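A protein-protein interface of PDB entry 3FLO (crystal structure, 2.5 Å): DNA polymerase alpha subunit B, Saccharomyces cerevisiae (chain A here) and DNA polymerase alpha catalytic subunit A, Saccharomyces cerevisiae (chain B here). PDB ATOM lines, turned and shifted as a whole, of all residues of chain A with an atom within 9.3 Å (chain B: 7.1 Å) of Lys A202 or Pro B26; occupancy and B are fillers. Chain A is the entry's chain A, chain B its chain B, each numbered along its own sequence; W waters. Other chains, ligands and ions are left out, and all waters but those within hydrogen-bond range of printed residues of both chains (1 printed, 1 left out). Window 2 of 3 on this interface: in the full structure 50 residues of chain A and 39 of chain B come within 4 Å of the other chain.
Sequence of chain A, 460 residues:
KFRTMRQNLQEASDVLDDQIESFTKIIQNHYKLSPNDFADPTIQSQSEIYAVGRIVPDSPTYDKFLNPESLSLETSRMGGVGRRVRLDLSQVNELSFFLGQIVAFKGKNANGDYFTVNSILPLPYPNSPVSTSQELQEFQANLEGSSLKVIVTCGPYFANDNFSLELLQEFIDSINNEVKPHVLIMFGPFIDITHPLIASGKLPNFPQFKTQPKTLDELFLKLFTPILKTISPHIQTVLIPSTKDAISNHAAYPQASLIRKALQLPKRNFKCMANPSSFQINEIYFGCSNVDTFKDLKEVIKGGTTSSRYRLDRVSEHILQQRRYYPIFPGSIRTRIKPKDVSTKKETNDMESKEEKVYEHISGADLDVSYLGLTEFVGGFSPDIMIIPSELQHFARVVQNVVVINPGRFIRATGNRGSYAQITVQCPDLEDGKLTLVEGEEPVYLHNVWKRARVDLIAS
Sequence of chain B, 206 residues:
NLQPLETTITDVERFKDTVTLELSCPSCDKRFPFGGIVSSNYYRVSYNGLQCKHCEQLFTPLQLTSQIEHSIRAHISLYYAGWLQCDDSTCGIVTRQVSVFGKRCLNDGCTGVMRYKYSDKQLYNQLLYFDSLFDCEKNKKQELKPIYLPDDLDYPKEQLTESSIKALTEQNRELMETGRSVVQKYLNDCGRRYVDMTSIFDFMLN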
ATOM      1  N   ASN A 160       9.999  -5.562 -31.641  1.00  0.00           N
ATOM      2  CA  ASN A 160       9.308  -6.626 -32.356  1.00  0.00           C
ATOM      3  C   ASN A 160       9.491  -8.032 -31.776  1.00  0.00           C
ATOM      4  O   ASN A 160       8.679  -8.944 -32.056  1.00  0.00           O
ATOM      5  CB  ASN A 160       9.770  -6.658 -33.820  1.00  0.00           C
ATOM      6  CG  ASN A 160       9.032  -5.626 -34.695  1.00  0.00           C
ATOM      7  OD1 ASN A 160       8.244  -4.830 -34.217  1.00  0.00           O
ATOM      8  ND2 ASN A 160       9.299  -5.658 -35.971  1.00  0.00           N
ATOM      9  N   ASP A 161      10.560  -8.228 -31.028  1.00  0.00           N
ATOM     10  CA  ASP A 161      10.865  -9.538 -30.536  1.00  0.00           C
ATOM     11  C   ASP A 161      10.748  -9.683 -28.998  1.00  0.00           C
ATOM     12  O   ASP A 161      11.209 -10.673 -28.473  1.00  0.00           O
ATOM     13  CB  ASP A 161      12.252  -9.974 -31.033  1.00  0.00           C
ATOM     14  CG  ASP A 161      13.379  -9.069 -30.542  1.00  0.00           C
ATOM     15  OD1 ASP A 161      13.129  -7.995 -29.972  1.00  0.00           O
ATOM     16  OD2 ASP A 161      14.551  -9.442 -30.725  1.00  0.00           O
ATOM     17  N   ASN A 162      10.131  -8.728 -28.306  1.00  0.00           N
ATOM     18  CA  ASN A 162       9.918  -8.854 -26.890  1.00  0.00           C
ATOM     19  C   ASN A 162       8.844  -7.896 -26.390  1.00  0.00           C
ATOM     20  O   ASN A 162       8.187  -7.267 -27.204  1.00  0.00           O
ATOM     21  CB  ASN A 162      11.252  -8.718 -26.156  1.00  0.00           C
ATOM     22  CG  ASN A 162      11.832  -7.338 -26.244  1.00  0.00           C
ATOM     23  OD1 ASN A 162      11.100  -6.323 -26.150  1.00  0.00           O
ATOM     24  ND2 ASN A 162      13.165  -7.274 -26.386  1.00  0.00           N
ATOM     25  N   PHE A 163       8.630  -7.820 -25.077  1.00  0.00           N
ATOM     26  CA  PHE A 163       7.587  -6.968 -24.508  1.00  0.00           C
ATOM     27  C   PHE A 163       8.169  -6.025 -23.476  1.00  0.00           C
ATOM     28  O   PHE A 163       7.516  -5.608 -22.538  1.00  0.00           O
ATOM     29  CB  PHE A 163       6.478  -7.859 -23.944  1.00  0.00           C
ATOM     30  CG  PHE A 163       5.746  -8.642 -25.021  1.00  0.00           C
ATOM     31  CD1 PHE A 163       6.181  -9.881 -25.401  1.00  0.00           C
ATOM     32  CD2 PHE A 163       4.702  -8.085 -25.705  1.00  0.00           C
ATOM     33  CE1 PHE A 163       5.530 -10.590 -26.419  1.00  0.00           C
ATOM     34  CE2 PHE A 163       4.057  -8.777 -26.720  1.00  0.00           C
ATOM     35  CZ  PHE A 163       4.463 -10.007 -27.078  1.00  0.00           C
ATOM     36  N   HIS A 195       2.095  -5.759 -34.847  1.00  0.00           N
ATOM     37  CA  HIS A 195       3.297  -6.312 -34.228  1.00  0.00           C
ATOM     38  C   HIS A 195       3.360  -7.819 -34.554  1.00  0.00           C
ATOM     39  O   HIS A 195       2.358  -8.517 -34.514  1.00  0.00           O
ATOM     40  CB  HIS A 195       3.257  -6.008 -32.753  1.00  0.00           C
ATOM     41  CG  HIS A 195       4.444  -6.492 -31.997  1.00  0.00           C
ATOM     42  ND1 HIS A 195       4.715  -7.841 -31.818  1.00  0.00           N
ATOM     43  CD2 HIS A 195       5.395  -5.817 -31.315  1.00  0.00           C
ATOM     44  CE1 HIS A 195       5.809  -7.965 -31.081  1.00  0.00           C
ATOM     45  NE2 HIS A 195       6.238  -6.755 -30.755  1.00  0.00           N
ATOM     46  N   PRO A 196       4.510  -8.297 -35.009  1.00  0.00           N
ATOM     47  CA  PRO A 196       4.555  -9.670 -35.519  1.00  0.00           C
ATOM     48  C   PRO A 196       4.262 -10.789 -34.528  1.00  0.00           C
ATOM     49  O   PRO A 196       3.774 -11.837 -34.957  1.00  0.00           O
ATOM     50  CB  PRO A 196       5.969  -9.800 -36.110  1.00  0.00           C
ATOM     51  CG  PRO A 196       6.757  -8.695 -35.542  1.00  0.00           C
ATOM     52  CD  PRO A 196       5.785  -7.586 -35.180  1.00  0.00           C
ATOM     53  N   LEU A 197       4.536 -10.602 -33.248  1.00  0.00           N
ATOM     54  CA  LEU A 197       4.167 -11.614 -32.261  1.00  0.00           C
ATOM     55  C   LEU A 197       2.653 -11.549 -31.989  1.00  0.00           C
ATOM     56  O   LEU A 197       2.007 -12.593 -31.811  1.00  0.00           O
ATOM     57  CB  LEU A 197       5.009 -11.465 -30.981  1.00  0.00           C
ATOM     58  CG  LEU A 197       6.556 -11.576 -31.118  1.00  0.00           C
ATOM     59  CD1 LEU A 197       7.297 -11.337 -29.782  1.00  0.00           C
ATOM     60  CD2 LEU A 197       7.021 -12.898 -31.710  1.00  0.00           C
ATOM     61  N   ILE A 198       2.104 -10.340 -31.966  1.00  0.00           N
ATOM     62  CA  ILE A 198       0.654 -10.141 -31.783  1.00  0.00           C
ATOM     63  C   ILE A 198      -0.052 -10.718 -32.980  1.00  0.00           C
ATOM     64  O   ILE A 198      -0.948 -11.528 -32.839  1.00  0.00           O
ATOM     65  CB  ILE A 198       0.293  -8.646 -31.600  1.00  0.00           C
ATOM     66  CG1 ILE A 198       0.567  -8.234 -30.162  1.00  0.00           C
ATOM     67  CG2 ILE A 198      -1.161  -8.411 -31.918  1.00  0.00           C
ATOM     68  CD1 ILE A 198       1.268  -7.006 -30.052  1.00  0.00           C
ATOM     69  N   ALA A 199       0.444 -10.408 -34.166  1.00  0.00           N
ATOM     70  CA  ALA A 199      -0.154 -10.898 -35.412  1.00  0.00           C
ATOM     71  C   ALA A 199      -0.143 -12.367 -35.445  1.00  0.00           C
ATOM     72  O   ALA A 199      -1.138 -12.941 -35.841  1.00  0.00           O
ATOM     73  CB  ALA A 199       0.580 -10.370 -36.656  1.00  0.00           C
ATOM     74  N   SER A 200       0.964 -13.014 -35.098  1.00  0.00           N
ATOM     75  CA  SER A 200       1.025 -14.476 -35.220  1.00  0.00           C
ATOM     76  C   SER A 200       0.397 -15.207 -34.019  1.00  0.00           C
ATOM     77  O   SER A 200       0.300 -16.430 -34.019  1.00  0.00           O
ATOM     78  CB  SER A 200       2.483 -14.971 -35.375  1.00  0.00           C
ATOM     79  OG  SER A 200       3.342 -14.549 -34.310  1.00  0.00           O
ATOM     80  N   GLY A 201       0.013 -14.479 -32.975  1.00  0.00           N
ATOM     81  CA  GLY A 201      -0.450 -15.134 -31.746  1.00  0.00           C
ATOM     82  C   GLY A 201       0.622 -15.790 -30.899  1.00  0.00           C
ATOM     83  O   GLY A 201       0.319 -16.592 -30.000  1.00  0.00           O
ATOM     84  N   LYS A 202       1.888 -15.482 -31.187  1.00  0.00           N
ATOM     85  CA  LYS A 202       3.009 -16.035 -30.390  1.00  0.00           C
ATOM     86  C   LYS A 202       3.148 -15.173 -29.183  1.00  0.00           C
ATOM     87  O   LYS A 202       4.075 -14.440 -29.072  1.00  0.00           O
ATOM     88  CB  LYS A 202       4.357 -16.013 -31.127  1.00  0.00           C
ATOM     89  CG  LYS A 202       4.471 -17.010 -32.274  1.00  0.00           C
ATOM     90  CD  LYS A 202       5.898 -17.060 -32.810  1.00  0.00           C
ATOM     91  CE  LYS A 202       6.066 -18.075 -33.912  1.00  0.00           C
ATOM     92  NZ  LYS A 202       6.285 -19.391 -33.326  1.00  0.00           N
ATOM     93  N   LEU A 203       2.196 -15.258 -28.276  1.00  0.00           N
ATOM     94  CA  LEU A 203       2.201 -14.463 -27.068  1.00  0.00           C
ATOM     95  C   LEU A 203       2.533 -15.377 -25.868  1.00  0.00           C
ATOM     96  O   LEU A 203       1.916 -16.451 -25.652  1.00  0.00           O
ATOM     97  CB  LEU A 203       0.870 -13.763 -26.900  1.00  0.00           C
ATOM     98  CG  LEU A 203       0.759 -12.583 -27.880  1.00  0.00           C
ATOM     99  CD1 LEU A 203      -0.605 -12.421 -28.471  1.00  0.00           C
ATOM    100  CD2 LEU A 203       1.168 -11.305 -27.196  1.00  0.00           C
ATOM    101  N   PRO A 204       3.542 -14.976 -25.104  1.00  0.00           N
ATOM    102  CA  PRO A 204       4.041 -15.804 -24.045  1.00  0.00           C
ATOM    103  C   PRO A 204       3.283 -15.616 -22.743  1.00  0.00           C
ATOM    104  O   PRO A 204       2.453 -14.704 -22.580  1.00  0.00           O
ATOM    105  CB  PRO A 204       5.467 -15.307 -23.897  1.00  0.00           C
ATOM    106  CG  PRO A 204       5.338 -13.814 -24.115  1.00  0.00           C
ATOM    107  CD  PRO A 204       4.263 -13.689 -25.174  1.00  0.00           C
ATOM    108  N   ASN A 205       3.565 -16.534 -21.845  1.00  0.00           N
ATOM    109  CA  ASN A 205       3.211 -16.406 -20.467  1.00  0.00           C
ATOM    110  C   ASN A 205       4.048 -15.328 -19.826  1.00  0.00           C
ATOM    111  O   ASN A 205       5.256 -15.309 -20.005  1.00  0.00           O
ATOM    112  CB  ASN A 205       3.509 -17.715 -19.787  1.00  0.00           C
ATOM    113  CG  ASN A 205       3.108 -17.704 -18.364  1.00  0.00           C
ATOM    114  OD1 ASN A 205       3.964 -17.699 -17.477  1.00  0.00           O
ATOM    115  ND2 ASN A 205       1.808 -17.654 -18.114  1.00  0.00           N
ATOM    116  N   PHE A 206       3.412 -14.433 -19.088  1.00  0.00           N
ATOM    117  CA  PHE A 206       4.137 -13.357 -18.374  1.00  0.00           C
ATOM    118  C   PHE A 206       4.273 -13.677 -16.889  1.00  0.00           C
ATOM    119  O   PHE A 206       3.315 -13.570 -16.116  1.00  0.00           O
ATOM    120  CB  PHE A 206       3.418 -12.026 -18.540  1.00  0.00           C
ATOM    121  CG  PHE A 206       3.402 -11.528 -19.959  1.00  0.00           C
ATOM    122  CD1 PHE A 206       4.464 -10.815 -20.462  1.00  0.00           C
ATOM    123  CD2 PHE A 206       2.336 -11.790 -20.786  1.00  0.00           C
ATOM    124  CE1 PHE A 206       4.468 -10.360 -21.790  1.00  0.00           C
ATOM    125  CE2 PHE A 206       2.337 -11.341 -22.095  1.00  0.00           C
ATOM    126  CZ  PHE A 206       3.409 -10.627 -22.600  1.00  0.00           C
ATOM    127  N   LEU A 216      -6.177  -8.771 -25.947  1.00  0.00           N
ATOM    128  CA  LEU A 216      -5.209  -7.660 -26.105  1.00  0.00           C
ATOM    129  C   LEU A 216      -5.575  -6.444 -25.228  1.00  0.00           C
ATOM    130  O   LEU A 216      -4.683  -5.783 -24.722  1.00  0.00           O
ATOM    131  CB  LEU A 216      -5.016  -7.254 -27.556  1.00  0.00           C
ATOM    132  CG  LEU A 216      -4.425  -8.371 -28.416  1.00  0.00           C
ATOM    133  CD1 LEU A 216      -4.418  -8.045 -29.945  1.00  0.00           C
ATOM    134  CD2 LEU A 216      -3.022  -8.700 -27.872  1.00  0.00           C
ATOM    135  N   LEU A 219      -4.101  -7.203 -22.071  1.00  0.00           N
ATOM    136  CA  LEU A 219      -2.664  -7.055 -22.142  1.00  0.00           C
ATOM    137  C   LEU A 219      -2.268  -5.596 -21.938  1.00  0.00           C
ATOM    138  O   LEU A 219      -1.281  -5.328 -21.222  1.00  0.00           O
ATOM    139  CB  LEU A 219      -2.122  -7.579 -23.451  1.00  0.00           C
ATOM    140  CG  LEU A 219      -0.601  -7.592 -23.593  1.00  0.00           C
ATOM    141  CD1 LEU A 219       0.158  -8.324 -22.472  1.00  0.00           C
ATOM    142  CD2 LEU A 219      -0.253  -8.165 -24.998  1.00  0.00           C
ATOM    143  N   SER B  24      -2.856 -19.827 -36.280  1.00  0.00           N
ATOM    144  CA  SER B  24      -1.538 -20.333 -36.390  1.00  0.00           C
ATOM    145  C   SER B  24      -1.113 -20.823 -35.004  1.00  0.00           C
ATOM    146  O   SER B  24      -1.427 -20.195 -34.001  1.00  0.00           O
ATOM    147  CB  SER B  24      -0.620 -19.245 -36.897  1.00  0.00           C
ATOM    148  OG  SER B  24       0.426 -19.845 -37.638  1.00  0.00           O
ATOM    149  N   CYS B  25      -0.420 -21.955 -34.957  1.00  0.00           N
ATOM    150  CA  CYS B  25      -0.030 -22.560 -33.676  1.00  0.00           C
ATOM    151  C   CYS B  25       1.183 -21.859 -33.111  1.00  0.00           C
ATOM    152  O   CYS B  25       2.188 -21.746 -33.788  1.00  0.00           O
ATOM    153  CB  CYS B  25       0.252 -24.065 -33.821  1.00  0.00           C
ATOM    154  SG  CYS B  25       1.036 -24.812 -32.340  1.00  0.00           S
ATOM    155  N   PRO B  26       1.088 -21.367 -31.872  1.00  0.00           N
ATOM    156  CA  PRO B  26       2.222 -20.638 -31.310  1.00  0.00           C
ATOM    157  C   PRO B  26       3.524 -21.417 -31.225  1.00  0.00           C
ATOM    158  O   PRO B  26       4.582 -20.788 -31.377  1.00  0.00           O
ATOM    159  CB  PRO B  26       1.725 -20.230 -29.920  1.00  0.00           C
ATOM    160  CG  PRO B  26       0.217 -20.331 -30.025  1.00  0.00           C
ATOM    161  CD  PRO B  26      -0.076 -21.383 -30.975  1.00  0.00           C
ATOM    162  N   SER B  27       3.478 -22.738 -30.964  1.00  0.00           N
ATOM    163  CA  SER B  27       4.712 -23.528 -30.817  1.00  0.00           C
ATOM    164  C   SER B  27       5.300 -23.876 -32.174  1.00  0.00           C
ATOM    165  O   SER B  27       6.483 -23.639 -32.415  1.00  0.00           O
ATOM    166  CB  SER B  27       4.546 -24.856 -30.030  1.00  0.00           C
ATOM    167  OG  SER B  27       3.640 -24.759 -28.930  1.00  0.00           O
ATOM    168  N   CYS B  28       4.496 -24.476 -33.045  1.00  0.00           N
ATOM    169  CA  CYS B  28       5.053 -25.123 -34.232  1.00  0.00           C
ATOM    170  C   CYS B  28       4.722 -24.413 -35.541  1.00  0.00           C
ATOM    171  O   CYS B  28       5.297 -24.743 -36.560  1.00  0.00           O
ATOM    172  CB  CYS B  28       4.594 -26.576 -34.281  1.00  0.00           C
ATOM    173  SG  CYS B  28       2.914 -26.784 -34.826  1.00  0.00           S
ATOM    174  N   ASP B  29       3.807 -23.447 -35.511  1.00  0.00           N
ATOM    175  CA  ASP B  29       3.518 -22.548 -36.635  1.00  0.00           C
ATOM    176  C   ASP B  29       2.617 -23.134 -37.701  1.00  0.00           C
ATOM    177  O   ASP B  29       2.347 -22.478 -38.692  1.00  0.00           O
ATOM    178  CB  ASP B  29       4.779 -21.997 -37.313  1.00  0.00           C
ATOM    179  CG  ASP B  29       5.630 -21.131 -36.390  1.00  0.00           C
ATOM    180  OD1 ASP B  29       5.131 -20.585 -35.373  1.00  0.00           O
ATOM    181  OD2 ASP B  29       6.824 -21.000 -36.714  1.00  0.00           O
ATOM    182  N   LYS B  30       2.101 -24.341 -37.492  1.00  0.00           N
ATOM    183  CA  LYS B  30       1.141 -24.904 -38.438  1.00  0.00           C
ATOM    184  C   LYS B  30      -0.122 -24.027 -38.463  1.00  0.00           C
ATOM    185  O   LYS B  30      -0.591 -23.559 -37.410  1.00  0.00           O
ATOM    186  CB  LYS B  30       0.814 -26.373 -38.069  1.00  0.00           C
ATOM    187  CG  LYS B  30       0.776 -27.390 -39.264  1.00  0.00           C
ATOM    188  CD  LYS B  30       2.166 -27.940 -39.552  1.00  0.00           C
ATOM    189  CE  LYS B  30       2.179 -28.986 -40.703  1.00  0.00           C
ATOM    190  NZ  LYS B  30       0.873 -29.782 -40.845  1.00  0.00           N
ATOM    191  N   PHE B  32      -4.156 -23.379 -39.650  1.00  0.00           N
ATOM    192  CA  PHE B  32      -5.368 -24.147 -39.881  1.00  0.00           C
ATOM    193  C   PHE B  32      -6.629 -23.337 -39.661  1.00  0.00           C
ATOM    194  O   PHE B  32      -6.618 -22.394 -38.883  1.00  0.00           O
ATOM    195  CB  PHE B  32      -5.372 -25.397 -38.991  1.00  0.00           C
ATOM    196  CG  PHE B  32      -5.312 -25.107 -37.526  1.00  0.00           C
ATOM    197  CD1 PHE B  32      -4.120 -25.211 -36.832  1.00  0.00           C
ATOM    198  CD2 PHE B  32      -6.463 -24.778 -36.818  1.00  0.00           C
ATOM    199  CE1 PHE B  32      -4.074 -24.944 -35.480  1.00  0.00           C
ATOM    200  CE2 PHE B  32      -6.414 -24.523 -35.455  1.00  0.00           C
ATOM    201  CZ  PHE B  32      -5.239 -24.604 -34.791  1.00  0.00           C
ATOM    202  N   CYS B  52      -3.366 -28.078 -30.488  1.00  0.00           N
ATOM    203  CA  CYS B  52      -2.786 -28.347 -31.769  1.00  0.00           C
ATOM    204  C   CYS B  52      -2.463 -29.819 -31.961  1.00  0.00           C
ATOM    205  O   CYS B  52      -1.723 -30.391 -31.156  1.00  0.00           O
ATOM    206  CB  CYS B  52      -1.500 -27.545 -31.880  1.00  0.00           C
ATOM    207  SG  CYS B  52      -0.519 -27.968 -33.293  1.00  0.00           S
ATOM    208  N   CYS B  55       1.652 -30.790 -32.840  1.00  0.00           N
ATOM    209  CA  CYS B  55       2.641 -30.765 -31.754  1.00  0.00           C
ATOM    210  C   CYS B  55       2.076 -30.934 -30.327  1.00  0.00           C
ATOM    211  O   CYS B  55       2.827 -30.918 -29.352  1.00  0.00           O
ATOM    212  CB  CYS B  55       3.443 -29.471 -31.840  1.00  0.00           C
ATOM    213  SG  CYS B  55       2.626 -28.029 -31.108  1.00  0.00           S
ATOM    214  N   GLN B  57       0.617 -28.942 -28.353  1.00  0.00           N
ATOM    215  CA  GLN B  57       0.625 -27.800 -27.463  1.00  0.00           C
ATOM    216  C   GLN B  57      -0.723 -27.112 -27.396  1.00  0.00           C
ATOM    217  O   GLN B  57      -1.443 -27.020 -28.393  1.00  0.00           O
ATOM    218  CB  GLN B  57       1.721 -26.799 -27.831  1.00  0.00           C
ATOM    219  CG  GLN B  57       3.207 -27.228 -27.351  1.00  0.00           C
ATOM    220  CD  GLN B  57       3.293 -27.699 -25.891  1.00  0.00           C
ATOM    221  OE1 GLN B  57       2.810 -27.019 -24.992  1.00  0.00           O
ATOM    222  NE2 GLN B  57       3.915 -28.870 -25.661  1.00  0.00           N
ATOM    223  N   LEU B  58      -1.063 -26.668 -26.188  1.00  0.00           N
ATOM    224  CA  LEU B  58      -2.328 -26.018 -25.890  1.00  0.00           C
ATOM    225  C   LEU B  58      -2.230 -24.547 -26.151  1.00  0.00           C
ATOM    226  O   LEU B  58      -1.281 -23.948 -25.717  1.00  0.00           O
ATOM    227  CB  LEU B  58      -2.607 -26.127 -24.401  1.00  0.00           C
ATOM    228  CG  LEU B  58      -3.343 -27.337 -23.884  1.00  0.00           C
ATOM    229  CD1 LEU B  58      -3.149 -27.387 -22.335  1.00  0.00           C
ATOM    230  CD2 LEU B  58      -4.826 -27.252 -24.321  1.00  0.00           C
ATOM    231  N   PHE B  59      -3.231 -23.959 -26.796  1.00  0.00           N
ATOM    232  CA  PHE B  59      -3.287 -22.505 -26.908  1.00  0.00           C
ATOM    233  C   PHE B  59      -3.667 -21.950 -25.555  1.00  0.00           C
ATOM    234  O   PHE B  59      -4.532 -22.487 -24.900  1.00  0.00           O
ATOM    235  CB  PHE B  59      -4.386 -22.051 -27.851  1.00  0.00           C
ATOM    236  CG  PHE B  59      -4.059 -22.198 -29.294  1.00  0.00           C
ATOM    237  CD1 PHE B  59      -3.762 -23.440 -29.834  1.00  0.00           C
ATOM    238  CD2 PHE B  59      -4.113 -21.085 -30.135  1.00  0.00           C
ATOM    239  CE1 PHE B  59      -3.472 -23.579 -31.169  1.00  0.00           C
ATOM    240  CE2 PHE B  59      -3.841 -21.202 -31.481  1.00  0.00           C
ATOM    241  CZ  PHE B  59      -3.510 -22.456 -32.012  1.00  0.00           C
ATOM    242  N   THR B  60      -3.082 -20.830 -25.174  1.00  0.00           N
ATOM    243  CA  THR B  60      -3.650 -20.048 -24.098  1.00  0.00           C
ATOM    244  C   THR B  60      -4.750 -19.179 -24.686  1.00  0.00           C
ATOM    245  O   THR B  60      -4.836 -18.979 -25.925  1.00  0.00           O
ATOM    246  CB  THR B  60      -2.616 -19.129 -23.477  1.00  0.00           C
ATOM    247  OG1 THR B  60      -2.209 -18.196 -24.478  1.00  0.00           O
ATOM    248  CG2 THR B  60      -1.427 -19.922 -22.981  1.00  0.00           C
ATOM    249  N   LEU B  62      -5.031 -15.868 -24.569  1.00  0.00           N
ATOM    250  CA  LEU B  62      -4.436 -14.723 -25.288  1.00  0.00           C
ATOM    251  C   LEU B  62      -3.883 -15.153 -26.635  1.00  0.00           C
ATOM    252  O   LEU B  62      -3.998 -14.432 -27.623  1.00  0.00           O
ATOM    253  CB  LEU B  62      -3.321 -14.092 -24.484  1.00  0.00           C
ATOM    254  CG  LEU B  62      -2.652 -12.845 -25.086  1.00  0.00           C
ATOM    255  CD1 LEU B  62      -3.626 -11.718 -25.288  1.00  0.00           C
ATOM    256  CD2 LEU B  62      -1.533 -12.395 -24.173  1.00  0.00           C
ATOM    257  N   GLN B  63      -3.294 -16.344 -26.708  1.00  0.00           N
ATOM    258  CA  GLN B  63      -2.827 -16.859 -28.010  1.00  0.00           C
ATOM    259  C   GLN B  63      -3.941 -17.071 -29.026  1.00  0.00           C
ATOM    260  O   GLN B  63      -3.684 -17.051 -30.236  1.00  0.00           O
ATOM    261  CB  GLN B  63      -2.067 -18.162 -27.825  1.00  0.00           C
ATOM    262  CG  GLN B  63      -0.734 -17.978 -27.176  1.00  0.00           C
ATOM    263  CD  GLN B  63      -0.069 -19.277 -26.712  1.00  0.00           C
ATOM    264  OE1 GLN B  63      -0.656 -20.355 -26.723  1.00  0.00           O
ATOM    265  NE2 GLN B  63       1.174 -19.155 -26.313  1.00  0.00           N
ATOM    266  N   LEU B  64      -5.163 -17.291 -28.553  1.00  0.00           N
ATOM    267  CA  LEU B  64      -6.301 -17.456 -29.456  1.00  0.00           C
ATOM    268  C   LEU B  64      -6.908 -16.111 -29.784  1.00  0.00           C
ATOM    269  O   LEU B  64      -7.186 -15.826 -30.921  1.00  0.00           O
ATOM    270  CB  LEU B  64      -7.379 -18.349 -28.840  1.00  0.00           C
ATOM    271  CG  LEU B  64      -8.699 -18.480 -29.577  1.00  0.00           C
ATOM    272  CD1 LEU B  64      -8.530 -19.192 -30.947  1.00  0.00           C
ATOM    273  CD2 LEU B  64      -9.759 -19.125 -28.725  1.00  0.00           C
ATOM    274  N   SER B  66      -5.795 -12.950 -29.525  1.00  0.00           N
ATOM    275  CA  SER B  66      -4.979 -12.022 -30.291  1.00  0.00           C
ATOM    276  C   SER B  66      -5.117 -12.316 -31.799  1.00  0.00           C
ATOM    277  O   SER B  66      -5.126 -11.403 -32.607  1.00  0.00           O
ATOM    278  CB  SER B  66      -3.533 -12.131 -29.860  1.00  0.00           C
ATOM    279  OG  SER B  66      -3.102 -13.440 -30.175  1.00  0.00           O
ATOM    280  N   GLN B  67      -5.270 -13.591 -32.155  1.00  0.00           N
ATOM    281  CA  GLN B  67      -5.442 -13.971 -33.554  1.00  0.00           C
ATOM    282  C   GLN B  67      -6.859 -13.665 -34.039  1.00  0.00           C
ATOM    283  O   GLN B  67      -7.064 -13.261 -35.198  1.00  0.00           O
ATOM    284  CB  GLN B  67      -5.083 -15.463 -33.787  1.00  0.00           C
ATOM    285  CG  GLN B  67      -3.630 -15.715 -33.490  1.00  0.00           C
ATOM    286  CD  GLN B  67      -3.157 -17.139 -33.780  1.00  0.00           C
ATOM    287  OE1 GLN B  67      -3.058 -17.529 -34.938  1.00  0.00           O
ATOM    288  NE2 GLN B  67      -2.845 -17.912 -32.726  1.00  0.00           N
HETATM  289  O   HOH W   1      -2.867 -15.360 -36.944  1.00  0.00           O
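Of chain B, only Pro B26 and Asp B29 come within 4 Å of Lys A202.
Pro B26 touches two residues of chain A.
Printed residues of chain B within 4 Å of Gly A201: Pro B26, Gln B63, Ser B66 and Gln B67.
No residue of chain A comes within 4 Å of Cys B25.
No residue of chain A comes within 4 Å of Ser B27.
Of the printed residues of chain A, Gln B67 touches Ser A200 and Gly A201.
Of the printed residues of chain A, Asp B29 touches Lys A202.
Of the printed residues of chain B, Ile A198 touches Ser B66 (3.9 Å).
Phe B32 touches none of the printed residues of chain A.
Cys B55 touches none of the printed residues of chain A.
The nearest residue of chain A that does not touch Pro B26 is Leu A203 (5.3 Å).
The nearest printed residue of chain B that does not touch Leu A216 is Gln B67 (6.0 Å).
The backbone carbonyl oxygen (O) of Pro B26 sits at hydrogen-bond distance from the side-chain amino group (NZ) of Lys A202 (2.9 Å).
NZ of Lys A202 is in salt-bridge range of OD1 of Asp B29, 2.6 Å away.
The backbone carbonyl oxygen (O) of Leu A203 sits at hydrogen-bond distance from the side-chain amide nitrogen (NE2) of Gln B63, at 2.9 Å.
Ile A198 touches Ser B66.
Gln B67 touches Ser A200.
Gly A201 touches Pro B26.
Gly A201 touches Gln B63 (O to CG, 3.3 Å).
Ser B66 touches Gly A201.
CG of Gln B67 touches CA of Gly A201, 3.7 Å away.
Leu A203 touches Leu B62 (CB to CD2, 3.9 Å).
Ser B66 touches Leu A203 (OG to CD1, 3.2 Å).
Leu B62 touches Leu A216.
Ser B66 touches Leu A216 (CB to CD2, 3.998 Å).
O of Gln B63 lies within hydrogen-bond range of NE2 of Gln B67 (2.8 Å).
O of Leu A197 sits at hydrogen-bond distance from OG of Ser A200, 3.4 Å away.
The backbone carbonyl oxygen (O) of Leu B62 is in hydrogen-bond range of the side-chain hydroxyl (OG) of Ser B66.
N of Thr B60 sits at hydrogen-bond distance from OE1 of Gln B63 (2.9 Å).
The backbone carbonyl oxygen of Pro A196 sits at hydrogen-bond distance from the side-chain hydroxyl of Ser A200.
N of Ser B24 is in hydrogen-bond range of OE1 of Gln B67.
Water W1 bridges OE1 of Gln B67 (3.0 Å) and O of Ala A199 (3.2 Å).
Printed residues of chain B that touch a printed residue of chain A: Pro B26, Asp B29, Leu B62, Gln B63, Ser B66 and Gln B67.
Hydrophobic or aromatic side chains of chain B within 4 Å of the printed part of chain A: Pro B26 and Leu B62.
Among the printed residues, 13 pairs touch across the chains.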
